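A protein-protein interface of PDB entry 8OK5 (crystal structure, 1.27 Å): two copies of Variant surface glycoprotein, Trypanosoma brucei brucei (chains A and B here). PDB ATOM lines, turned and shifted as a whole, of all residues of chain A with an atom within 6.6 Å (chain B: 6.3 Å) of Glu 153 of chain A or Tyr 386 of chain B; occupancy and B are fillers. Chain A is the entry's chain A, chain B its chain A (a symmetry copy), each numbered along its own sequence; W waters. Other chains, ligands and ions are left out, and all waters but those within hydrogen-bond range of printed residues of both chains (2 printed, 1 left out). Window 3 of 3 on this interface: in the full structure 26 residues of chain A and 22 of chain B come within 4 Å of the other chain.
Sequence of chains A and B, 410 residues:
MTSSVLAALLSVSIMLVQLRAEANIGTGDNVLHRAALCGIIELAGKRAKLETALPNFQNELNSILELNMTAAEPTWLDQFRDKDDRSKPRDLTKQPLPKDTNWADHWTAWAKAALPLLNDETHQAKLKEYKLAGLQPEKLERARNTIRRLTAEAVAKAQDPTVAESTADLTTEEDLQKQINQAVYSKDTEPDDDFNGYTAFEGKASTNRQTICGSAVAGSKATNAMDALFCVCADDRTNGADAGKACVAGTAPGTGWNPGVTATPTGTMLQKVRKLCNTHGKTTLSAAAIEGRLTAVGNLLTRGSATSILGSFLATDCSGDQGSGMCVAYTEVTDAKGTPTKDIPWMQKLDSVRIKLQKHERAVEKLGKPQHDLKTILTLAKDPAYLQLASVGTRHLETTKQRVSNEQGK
OE2 of Glu 153 of chain A lies within hydrogen-bond range of OH of Tyr 386 of chain B.
The side-chain carboxylate (OD1) of Asp 383 of chain B lies within hydrogen-bond range of the backbone NH (N) of Tyr 386 of chain B, 3.4 Å away. The guanidinium group (NH2) of Arg 149 of chain A lies within hydrogen-bond range of the side-chain hydroxyl (OH) of Tyr 386 of chain A (3.0 Å). The guanidinium group of Arg 149 of chain B sits at hydrogen-bond distance from the side-chain hydroxyl of Tyr 386 of chain B (3.0 Å). The guanidinium group (NH1) of Arg 149 of chain A lies within salt-bridge range of the side-chain carboxylate (OE2) of Glu 153 of chain A (3.0 Å).
Among the printed residues, merely in contact across the chains: Ala 152 of chain A with Tyr 386 of chain B (3.5 Å), Lys 157 of chain A with Thr 376 of chain B (3.7 Å), Arg 149 of chain A with Tyr 386 of chain B (3.8 Å), Arg 148 of chain A with Leu 389 of chain B (3.8 Å), Ala 152 of chain A with Leu 380 of chain B (3.8 Å), Ala 156 of chain A with Leu 380 of chain B (3.8 Å), Ala 156 of chain A with Thr 376 of chain B (3.9 Å), Arg 149 of chain A with Leu 389 of chain B (3.9 Å) and Glu 153 of chain A with Leu 380 of chain B (3.9 Å).
Glu 153 of chain A touches two residues of chain B. Of the printed residues of chain B, Lys 157 of chain A touches Thr 376 (3.7 Å). Of the printed residues of chain B, Arg 149 of chain A touches Tyr 386 and Leu 389. Printed residues of chain A within 4 Å of Leu 380 of chain B: Ala 152 (3.8 Å), Glu 153 (3.9 Å) and Ala 156 (3.8 Å). Printed residues of chain A within 4 Å of Thr 376 of chain B: Ala 156 and Lys 157. The nearest residue of chain A that does not touch Tyr 386 of chain B is Arg 148 of chain A (5.5 Å).
Hydrophobic or aromatic side chains of chain A that line the printed part of chain B: Ala 152 and Ala 156. Among the printed residues, 10 pairs touch across the chains.
Arg 149 of chain A touches Tyr 386 of chain B, but with the chains exchanged Tyr 386 of chain A does not touch Arg 149 of chain B (8.5 Å). Of the 10 pairs that touch across the chains among the printed residues, none has its exchanged pair printed and touching as well.
Water W2 lies within hydrogen-bond range of OE2 of Glu 153 of chain A (2.8 Å) and NH1 of Arg 149 of chain B (2.9 Å). Water W1 lies within hydrogen-bond range of NZ of Lys 157 of chain A (2.8 Å) and OG1 of Thr 376 of chain B (3.1 Å).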
ATOM      1  N   ARG A 148       1.748  -9.924 -21.118  1.00  0.00           N
ATOM      2  CA  ARG A 148       2.567  -9.485 -19.957  1.00  0.00           C
ATOM      3  C   ARG A 148       3.537 -10.609 -19.593  1.00  0.00           C
ATOM      4  O   ARG A 148       4.659 -10.323 -19.294  1.00  0.00           O
ATOM      5  CB  ARG A 148       1.646  -9.133 -18.791  1.00  0.00           C
ATOM      6  CG  ARG A 148       1.007  -7.764 -18.959  1.00  0.00           C
ATOM      7  CD  ARG A 148       0.021  -7.465 -17.857  1.00  0.00           C
ATOM      8  NE  ARG A 148       0.717  -7.101 -16.636  1.00  0.00           N
ATOM      9  CZ  ARG A 148       0.200  -6.364 -15.664  1.00  0.00           C
ATOM     10  NH1 ARG A 148      -1.063  -5.987 -15.718  1.00  0.00           N
ATOM     11  NH2 ARG A 148       0.958  -6.001 -14.648  1.00  0.00           N
ATOM     12  N   ARG A 149       3.072 -11.847 -19.678  1.00  0.00           N
ATOM     13  CA  ARG A 149       3.911 -13.021 -19.358  1.00  0.00           C
ATOM     14  C   ARG A 149       5.022 -13.156 -20.404  1.00  0.00           C
ATOM     15  O   ARG A 149       6.152 -13.338 -20.016  1.00  0.00           O
ATOM     16  CB  ARG A 149       3.064 -14.298 -19.345  1.00  0.00           C
ATOM     17  CG  ARG A 149       3.876 -15.557 -19.091  1.00  0.00           C
ATOM     18  CD  ARG A 149       3.039 -16.819 -19.090  1.00  0.00           C
ATOM     19  NE  ARG A 149       2.403 -17.054 -20.377  1.00  0.00           N
ATOM     20  CZ  ARG A 149       2.980 -17.631 -21.421  1.00  0.00           C
ATOM     21  NH1 ARG A 149       4.289 -17.776 -21.462  1.00  0.00           N
ATOM     22  NH2 ARG A 149       2.239 -18.048 -22.432  1.00  0.00           N
ATOM     23  N   LEU A 150       4.676 -13.097 -21.694  1.00  0.00           N
ATOM     24  CA  LEU A 150       5.681 -13.193 -22.757  1.00  0.00           C
ATOM     25  C   LEU A 150       6.689 -12.056 -22.669  1.00  0.00           C
ATOM     26  O   LEU A 150       7.884 -12.254 -22.940  1.00  0.00           O
ATOM     27  CB  LEU A 150       4.965 -13.153 -24.099  1.00  0.00           C
ATOM     28  CG  LEU A 150       4.212 -14.397 -24.550  1.00  0.00           C
ATOM     29  CD1 LEU A 150       3.421 -14.052 -25.837  1.00  0.00           C
ATOM     30  CD2 LEU A 150       5.162 -15.500 -24.799  1.00  0.00           C
ATOM     31  N   THR A 151       6.241 -10.883 -22.335  1.00  0.00           N
ATOM     32  CA  THR A 151       7.132  -9.713 -22.220  1.00  0.00           C
ATOM     33  C   THR A 151       8.132  -9.907 -21.085  1.00  0.00           C
ATOM     34  O   THR A 151       9.330  -9.646 -21.254  1.00  0.00           O
ATOM     35  CB  THR A 151       6.339  -8.413 -22.029  1.00  0.00           C
ATOM     36  OG1 THR A 151       5.495  -8.253 -23.154  1.00  0.00           O
ATOM     37  CG2 THR A 151       7.254  -7.237 -21.974  1.00  0.00           C
ATOM     38  N   ALA A 152       7.670 -10.396 -19.922  1.00  0.00           N
ATOM     39  CA  ALA A 152       8.577 -10.666 -18.816  1.00  0.00           C
ATOM     40  C   ALA A 152       9.625 -11.713 -19.219  1.00  0.00           C
ATOM     41  O   ALA A 152      10.798 -11.618 -18.849  1.00  0.00           O
ATOM     42  CB  ALA A 152       7.759 -11.154 -17.607  1.00  0.00           C
ATOM     43  N   GLU A 153       9.192 -12.721 -19.963  1.00  0.00           N
ATOM     44  CA  GLU A 153      10.131 -13.756 -20.419  1.00  0.00           C
ATOM     45  C   GLU A 153      11.140 -13.203 -21.394  1.00  0.00           C
ATOM     46  O   GLU A 153      12.340 -13.522 -21.304  1.00  0.00           O
ATOM     47  CB  GLU A 153       9.344 -14.928 -21.010  1.00  0.00           C
ATOM     48  CG  GLU A 153       8.517 -15.637 -19.972  1.00  0.00           C
ATOM     49  CD  GLU A 153       7.409 -16.520 -20.516  1.00  0.00           C
ATOM     50  OE1 GLU A 153       7.379 -16.730 -21.748  1.00  0.00           O
ATOM     51  OE2 GLU A 153       6.565 -16.990 -19.738  1.00  0.00           O
ATOM     52  N   ALA A 154      10.684 -12.311 -22.272  1.00  0.00           N
ATOM     53  CA  ALA A 154      11.624 -11.676 -23.208  1.00  0.00           C
ATOM     54  C   ALA A 154      12.699 -10.895 -22.471  1.00  0.00           C
ATOM     55  O   ALA A 154      13.896 -10.990 -22.821  1.00  0.00           O
ATOM     56  CB  ALA A 154      10.864 -10.765 -24.174  1.00  0.00           C
ATOM     57  N   VAL A 155      12.300 -10.105 -21.484  1.00  0.00           N
ATOM     58  CA  VAL A 155      13.269  -9.318 -20.721  1.00  0.00           C
ATOM     59  C   VAL A 155      14.221 -10.225 -19.963  1.00  0.00           C
ATOM     60  O   VAL A 155      15.430 -10.015 -19.977  1.00  0.00           O
ATOM     61  CB  VAL A 155      12.518  -8.354 -19.764  1.00  0.00           C
ATOM     62  CG1 VAL A 155      13.485  -7.710 -18.746  1.00  0.00           C
ATOM     63  CG2 VAL A 155      11.747  -7.305 -20.546  1.00  0.00           C
ATOM     64  N   ALA A 156      13.713 -11.274 -19.368  1.00  0.00           N
ATOM     65  CA  ALA A 156      14.580 -12.177 -18.612  1.00  0.00           C
ATOM     66  C   ALA A 156      15.601 -12.835 -19.525  1.00  0.00           C
ATOM     67  O   ALA A 156      16.757 -13.038 -19.132  1.00  0.00           O
ATOM     68  CB  ALA A 156      13.750 -13.207 -17.855  1.00  0.00           C
ATOM     69  N   LYS A 157      15.207 -13.155 -20.763  1.00  0.00           N
ATOM     70  CA  LYS A 157      16.151 -13.800 -21.678  1.00  0.00           C
ATOM     71  C   LYS A 157      17.172 -12.807 -22.220  1.00  0.00           C
ATOM     72  O   LYS A 157      18.366 -13.139 -22.380  1.00  0.00           O
ATOM     73  CB  LYS A 157      15.381 -14.361 -22.864  1.00  0.00           C
ATOM     74  CG  LYS A 157      14.549 -15.543 -22.528  1.00  0.00           C
ATOM     75  CD  LYS A 157      13.528 -15.791 -23.630  1.00  0.00           C
ATOM     76  CE  LYS A 157      12.750 -17.018 -23.455  1.00  0.00           C
ATOM     77  NZ  LYS A 157      13.569 -18.236 -23.567  1.00  0.00           N
ATOM     78  N   ALA A 158      16.738 -11.595 -22.543  1.00  0.00           N
ATOM     79  CA  ALA A 158      17.601 -10.615 -23.212  1.00  0.00           C
ATOM     80  C   ALA A 158      18.380  -9.754 -22.238  1.00  0.00           C
ATOM     81  O   ALA A 158      19.440  -9.228 -22.613  1.00  0.00           O
ATOM     82  CB  ALA A 158      16.779  -9.718 -24.138  1.00  0.00           C
ATOM     83  N   LEU A 374      13.640 -14.218 -28.949  1.00  0.00           N
ATOM     84  CA  LEU A 374      12.839 -13.005 -29.051  1.00  0.00           C
ATOM     85  C   LEU A 374      11.992 -13.023 -30.319  1.00  0.00           C
ATOM     86  O   LEU A 374      10.847 -12.555 -30.312  1.00  0.00           O
ATOM     87  CB  LEU A 374      13.704 -11.757 -28.982  1.00  0.00           C
ATOM     88  CG  LEU A 374      14.244 -11.375 -27.610  1.00  0.00           C
ATOM     89  CD1 LEU A 374      14.824  -9.958 -27.680  1.00  0.00           C
ATOM     90  CD2 LEU A 374      13.231 -11.466 -26.551  1.00  0.00           C
ATOM     91  N   ILE A 377       9.019 -15.173 -29.490  1.00  0.00           N
ATOM     92  CA  ILE A 377       8.056 -14.516 -28.617  1.00  0.00           C
ATOM     93  C   ILE A 377       7.246 -13.503 -29.403  1.00  0.00           C
ATOM     94  O   ILE A 377       6.034 -13.398 -29.228  1.00  0.00           O
ATOM     95  CB  ILE A 377       8.788 -13.852 -27.432  1.00  0.00           C
ATOM     96  CG1 ILE A 377       9.261 -14.940 -26.459  1.00  0.00           C
ATOM     97  CG2 ILE A 377       7.880 -12.856 -26.724  1.00  0.00           C
ATOM     98  CD1 ILE A 377      10.162 -14.394 -25.360  1.00  0.00           C
ATOM     99  N   TYR A 386      -3.207 -17.742 -30.106  1.00  0.00           N
ATOM    100  CA  TYR A 386      -2.358 -18.147 -28.994  1.00  0.00           C
ATOM    101  C   TYR A 386      -2.653 -17.307 -27.762  1.00  0.00           C
ATOM    102  O   TYR A 386      -2.667 -17.804 -26.644  1.00  0.00           O
ATOM    103  CB  TYR A 386      -0.872 -18.051 -29.383  1.00  0.00           C
ATOM    104  CG  TYR A 386       0.066 -18.399 -28.247  1.00  0.00           C
ATOM    105  CD1 TYR A 386       0.392 -19.705 -27.975  1.00  0.00           C
ATOM    106  CD2 TYR A 386       0.627 -17.415 -27.435  1.00  0.00           C
ATOM    107  CE1 TYR A 386       1.274 -20.010 -26.946  1.00  0.00           C
ATOM    108  CE2 TYR A 386       1.469 -17.694 -26.420  1.00  0.00           C
ATOM    109  CZ  TYR A 386       1.822 -18.995 -26.161  1.00  0.00           C
ATOM    110  OH  TYR A 386       2.651 -19.275 -25.134  1.00  0.00           O
ATOM    111  N   THR B 146       3.160 -21.343 -10.476  1.00  0.00           N
ATOM    112  CA  THR B 146       4.103 -20.935 -11.507  1.00  0.00           C
ATOM    113  C   THR B 146       5.452 -21.587 -11.281  1.00  0.00           C
ATOM    114  O   THR B 146       6.140 -22.025 -12.208  1.00  0.00           O
ATOM    115  CB  THR B 146       4.234 -19.412 -11.532  1.00  0.00           C
ATOM    116  OG1 THR B 146       2.924 -18.877 -11.768  1.00  0.00           O
ATOM    117  CG2 THR B 146       5.189 -19.010 -12.648  1.00  0.00           C
ATOM    118  N   ARG B 149       5.625 -25.155 -12.445  1.00  0.00           N
ATOM    119  CA  ARG B 149       5.679 -25.196 -13.921  1.00  0.00           C
ATOM    120  C   ARG B 149       7.099 -24.867 -14.391  1.00  0.00           C
ATOM    121  O   ARG B 149       7.605 -25.583 -15.224  1.00  0.00           O
ATOM    122  CB  ARG B 149       4.695 -24.186 -14.523  1.00  0.00           C
ATOM    123  CG  ARG B 149       4.747 -24.124 -16.039  1.00  0.00           C
ATOM    124  CD  ARG B 149       3.783 -23.118 -16.631  1.00  0.00           C
ATOM    125  NE  ARG B 149       4.082 -21.758 -16.204  1.00  0.00           N
ATOM    126  CZ  ARG B 149       4.993 -20.968 -16.753  1.00  0.00           C
ATOM    127  NH1 ARG B 149       5.910 -21.466 -17.557  1.00  0.00           N
ATOM    128  NH2 ARG B 149       4.987 -19.675 -16.482  1.00  0.00           N
ATOM    129  N   LEU B 150       7.692 -23.785 -13.876  1.00  0.00           N
ATOM    130  CA  LEU B 150       9.060 -23.415 -14.253  1.00  0.00           C
ATOM    131  C   LEU B 150      10.052 -24.503 -13.875  1.00  0.00           C
ATOM    132  O   LEU B 150      11.020 -24.755 -14.610  1.00  0.00           O
ATOM    133  CB  LEU B 150       9.417 -22.114 -13.547  1.00  0.00           C
ATOM    134  CG  LEU B 150       8.805 -20.821 -14.070  1.00  0.00           C
ATOM    135  CD1 LEU B 150       9.162 -19.678 -13.086  1.00  0.00           C
ATOM    136  CD2 LEU B 150       9.321 -20.528 -15.422  1.00  0.00           C
ATOM    137  N   THR B 376      17.612 -17.938 -17.041  1.00  0.00           N
ATOM    138  CA  THR B 376      16.361 -17.225 -17.310  1.00  0.00           C
ATOM    139  C   THR B 376      15.272 -17.670 -16.354  1.00  0.00           C
ATOM    140  O   THR B 376      14.511 -16.852 -15.816  1.00  0.00           O
ATOM    141  CB  THR B 376      15.906 -17.507 -18.746  1.00  0.00           C
ATOM    142  OG1 THR B 376      16.884 -17.038 -19.654  1.00  0.00           O
ATOM    143  CG2 THR B 376      14.538 -16.802 -19.015  1.00  0.00           C
ATOM    144  N   LEU B 380      13.120 -15.558 -13.537  1.00  0.00           N
ATOM    145  CA  LEU B 380      11.671 -15.489 -13.453  1.00  0.00           C
ATOM    146  C   LEU B 380      11.152 -16.003 -12.102  1.00  0.00           C
ATOM    147  O   LEU B 380      10.139 -15.477 -11.573  1.00  0.00           O
ATOM    148  CB  LEU B 380      11.071 -16.253 -14.634  1.00  0.00           C
ATOM    149  CG  LEU B 380      11.270 -15.627 -16.009  1.00  0.00           C
ATOM    150  CD1 LEU B 380      10.931 -16.671 -17.030  1.00  0.00           C
ATOM    151  CD2 LEU B 380      10.483 -14.358 -16.218  1.00  0.00           C
ATOM    152  N   ALA B 381      11.755 -17.096 -11.578  1.00  0.00           N
ATOM    153  CA  ALA B 381      11.236 -17.718 -10.375  1.00  0.00           C
ATOM    154  C   ALA B 381      11.448 -16.829  -9.168  1.00  0.00           C
ATOM    155  O   ALA B 381      10.715 -16.976  -8.171  1.00  0.00           O
ATOM    156  CB  ALA B 381      11.922 -19.052 -10.139  1.00  0.00           C
ATOM    157  N   ASP B 383      11.182 -13.484  -9.417  1.00  0.00           N
ATOM    158  CA  ASP B 383      10.455 -12.261  -9.714  1.00  0.00           C
ATOM    159  C   ASP B 383       9.046 -12.388  -9.151  1.00  0.00           C
ATOM    160  O   ASP B 383       8.187 -13.067  -9.748  1.00  0.00           O
ATOM    161  CB  ASP B 383      10.416 -12.032 -11.233  1.00  0.00           C
ATOM    162  CG  ASP B 383       9.575 -10.838 -11.644  1.00  0.00           C
ATOM    163  OD1 ASP B 383       8.987 -10.173 -10.777  1.00  0.00           O
ATOM    164  OD2 ASP B 383       9.494 -10.555 -12.872  1.00  0.00           O
ATOM    165  N   PRO B 384       8.744 -11.777  -7.995  1.00  0.00           N
ATOM    166  CA  PRO B 384       7.412 -11.987  -7.414  1.00  0.00           C
ATOM    167  C   PRO B 384       6.257 -11.583  -8.307  1.00  0.00           C
ATOM    168  O   PRO B 384       5.218 -12.263  -8.347  1.00  0.00           O
ATOM    169  CB  PRO B 384       7.488 -11.141  -6.123  1.00  0.00           C
ATOM    170  CG  PRO B 384       8.982 -11.153  -5.751  1.00  0.00           C
ATOM    171  CD  PRO B 384       9.622 -10.979  -7.120  1.00  0.00           C
ATOM    172  N   ALA B 385       6.421 -10.504  -9.089  1.00  0.00           N
ATOM    173  CA  ALA B 385       5.354 -10.046  -9.976  1.00  0.00           C
ATOM    174  C   ALA B 385       5.054 -11.064 -11.080  1.00  0.00           C
ATOM    175  O   ALA B 385       3.902 -11.290 -11.440  1.00  0.00           O
ATOM    176  CB  ALA B 385       5.689  -8.669 -10.521  1.00  0.00           C
ATOM    177  N   TYR B 386       6.085 -11.661 -11.665  1.00  0.00           N
ATOM    178  CA  TYR B 386       5.864 -12.672 -12.690  1.00  0.00           C
ATOM    179  C   TYR B 386       5.112 -13.861 -12.115  1.00  0.00           C
ATOM    180  O   TYR B 386       4.245 -14.433 -12.760  1.00  0.00           O
ATOM    181  CB  TYR B 386       7.200 -13.113 -13.313  1.00  0.00           C
ATOM    182  CG  TYR B 386       7.044 -14.211 -14.343  1.00  0.00           C
ATOM    183  CD1 TYR B 386       6.724 -13.917 -15.646  1.00  0.00           C
ATOM    184  CD2 TYR B 386       7.211 -15.554 -14.012  1.00  0.00           C
ATOM    185  CE1 TYR B 386       6.609 -14.929 -16.588  1.00  0.00           C
ATOM    186  CE2 TYR B 386       7.084 -16.552 -14.909  1.00  0.00           C
ATOM    187  CZ  TYR B 386       6.794 -16.262 -16.219  1.00  0.00           C
ATOM    188  OH  TYR B 386       6.648 -17.263 -17.113  1.00  0.00           O
ATOM    189  N   LEU B 387       5.458 -14.264 -10.905  1.00  0.00           N
ATOM    190  CA  LEU B 387       4.866 -15.484 -10.345  1.00  0.00           C
ATOM    191  C   LEU B 387       3.366 -15.312 -10.157  1.00  0.00           C
ATOM    192  O   LEU B 387       2.590 -16.263 -10.343  1.00  0.00           O
ATOM    193  CB  LEU B 387       5.509 -15.857  -9.017  1.00  0.00           C
ATOM    194  CG  LEU B 387       6.973 -16.283  -9.063  1.00  0.00           C
ATOM    195  CD1 LEU B 387       7.449 -16.788  -7.715  1.00  0.00           C
ATOM    196  CD2 LEU B 387       7.172 -17.342 -10.141  1.00  0.00           C
ATOM    197  N   GLN B 388       2.953 -14.104  -9.804  1.00  0.00           N
ATOM    198  CA  GLN B 388       1.528 -13.836  -9.622  1.00  0.00           C
ATOM    199  C   GLN B 388       0.818 -13.749 -10.964  1.00  0.00           C
ATOM    200  O   GLN B 388      -0.316 -14.206 -11.108  1.00  0.00           O
ATOM    201  CB  GLN B 388       1.348 -12.527  -8.832  1.00  0.00           C
ATOM    202  CG  GLN B 388       1.882 -12.596  -7.395  1.00  0.00           C
ATOM    203  CD  GLN B 388       1.262 -13.713  -6.556  1.00  0.00           C
ATOM    204  OE1 GLN B 388       0.047 -13.898  -6.525  1.00  0.00           O
ATOM    205  NE2 GLN B 388       2.106 -14.459  -5.874  1.00  0.00           N
ATOM    206  N   LEU B 389       1.492 -13.192 -11.961  1.00  0.00           N
ATOM    207  CA  LEU B 389       0.959 -13.037 -13.289  1.00  0.00           C
ATOM    208  C   LEU B 389       0.409 -14.351 -13.810  1.00  0.00           C
ATOM    209  O   LEU B 389      -0.618 -14.386 -14.485  1.00  0.00           O
ATOM    210  CB  LEU B 389       2.087 -12.574 -14.204  1.00  0.00           C
ATOM    211  CG  LEU B 389       1.859 -11.440 -15.176  1.00  0.00           C
ATOM    212  CD1 LEU B 389       1.323 -10.199 -14.486  1.00  0.00           C
ATOM    213  CD2 LEU B 389       3.198 -11.136 -15.861  1.00  0.00           C
HETATM  214  O   HOH W   1      15.890 -18.762 -22.074  1.00  0.00           O
HETATM  215  O   HOH W   2       6.726 -19.752 -19.746  1.00  0.00           O
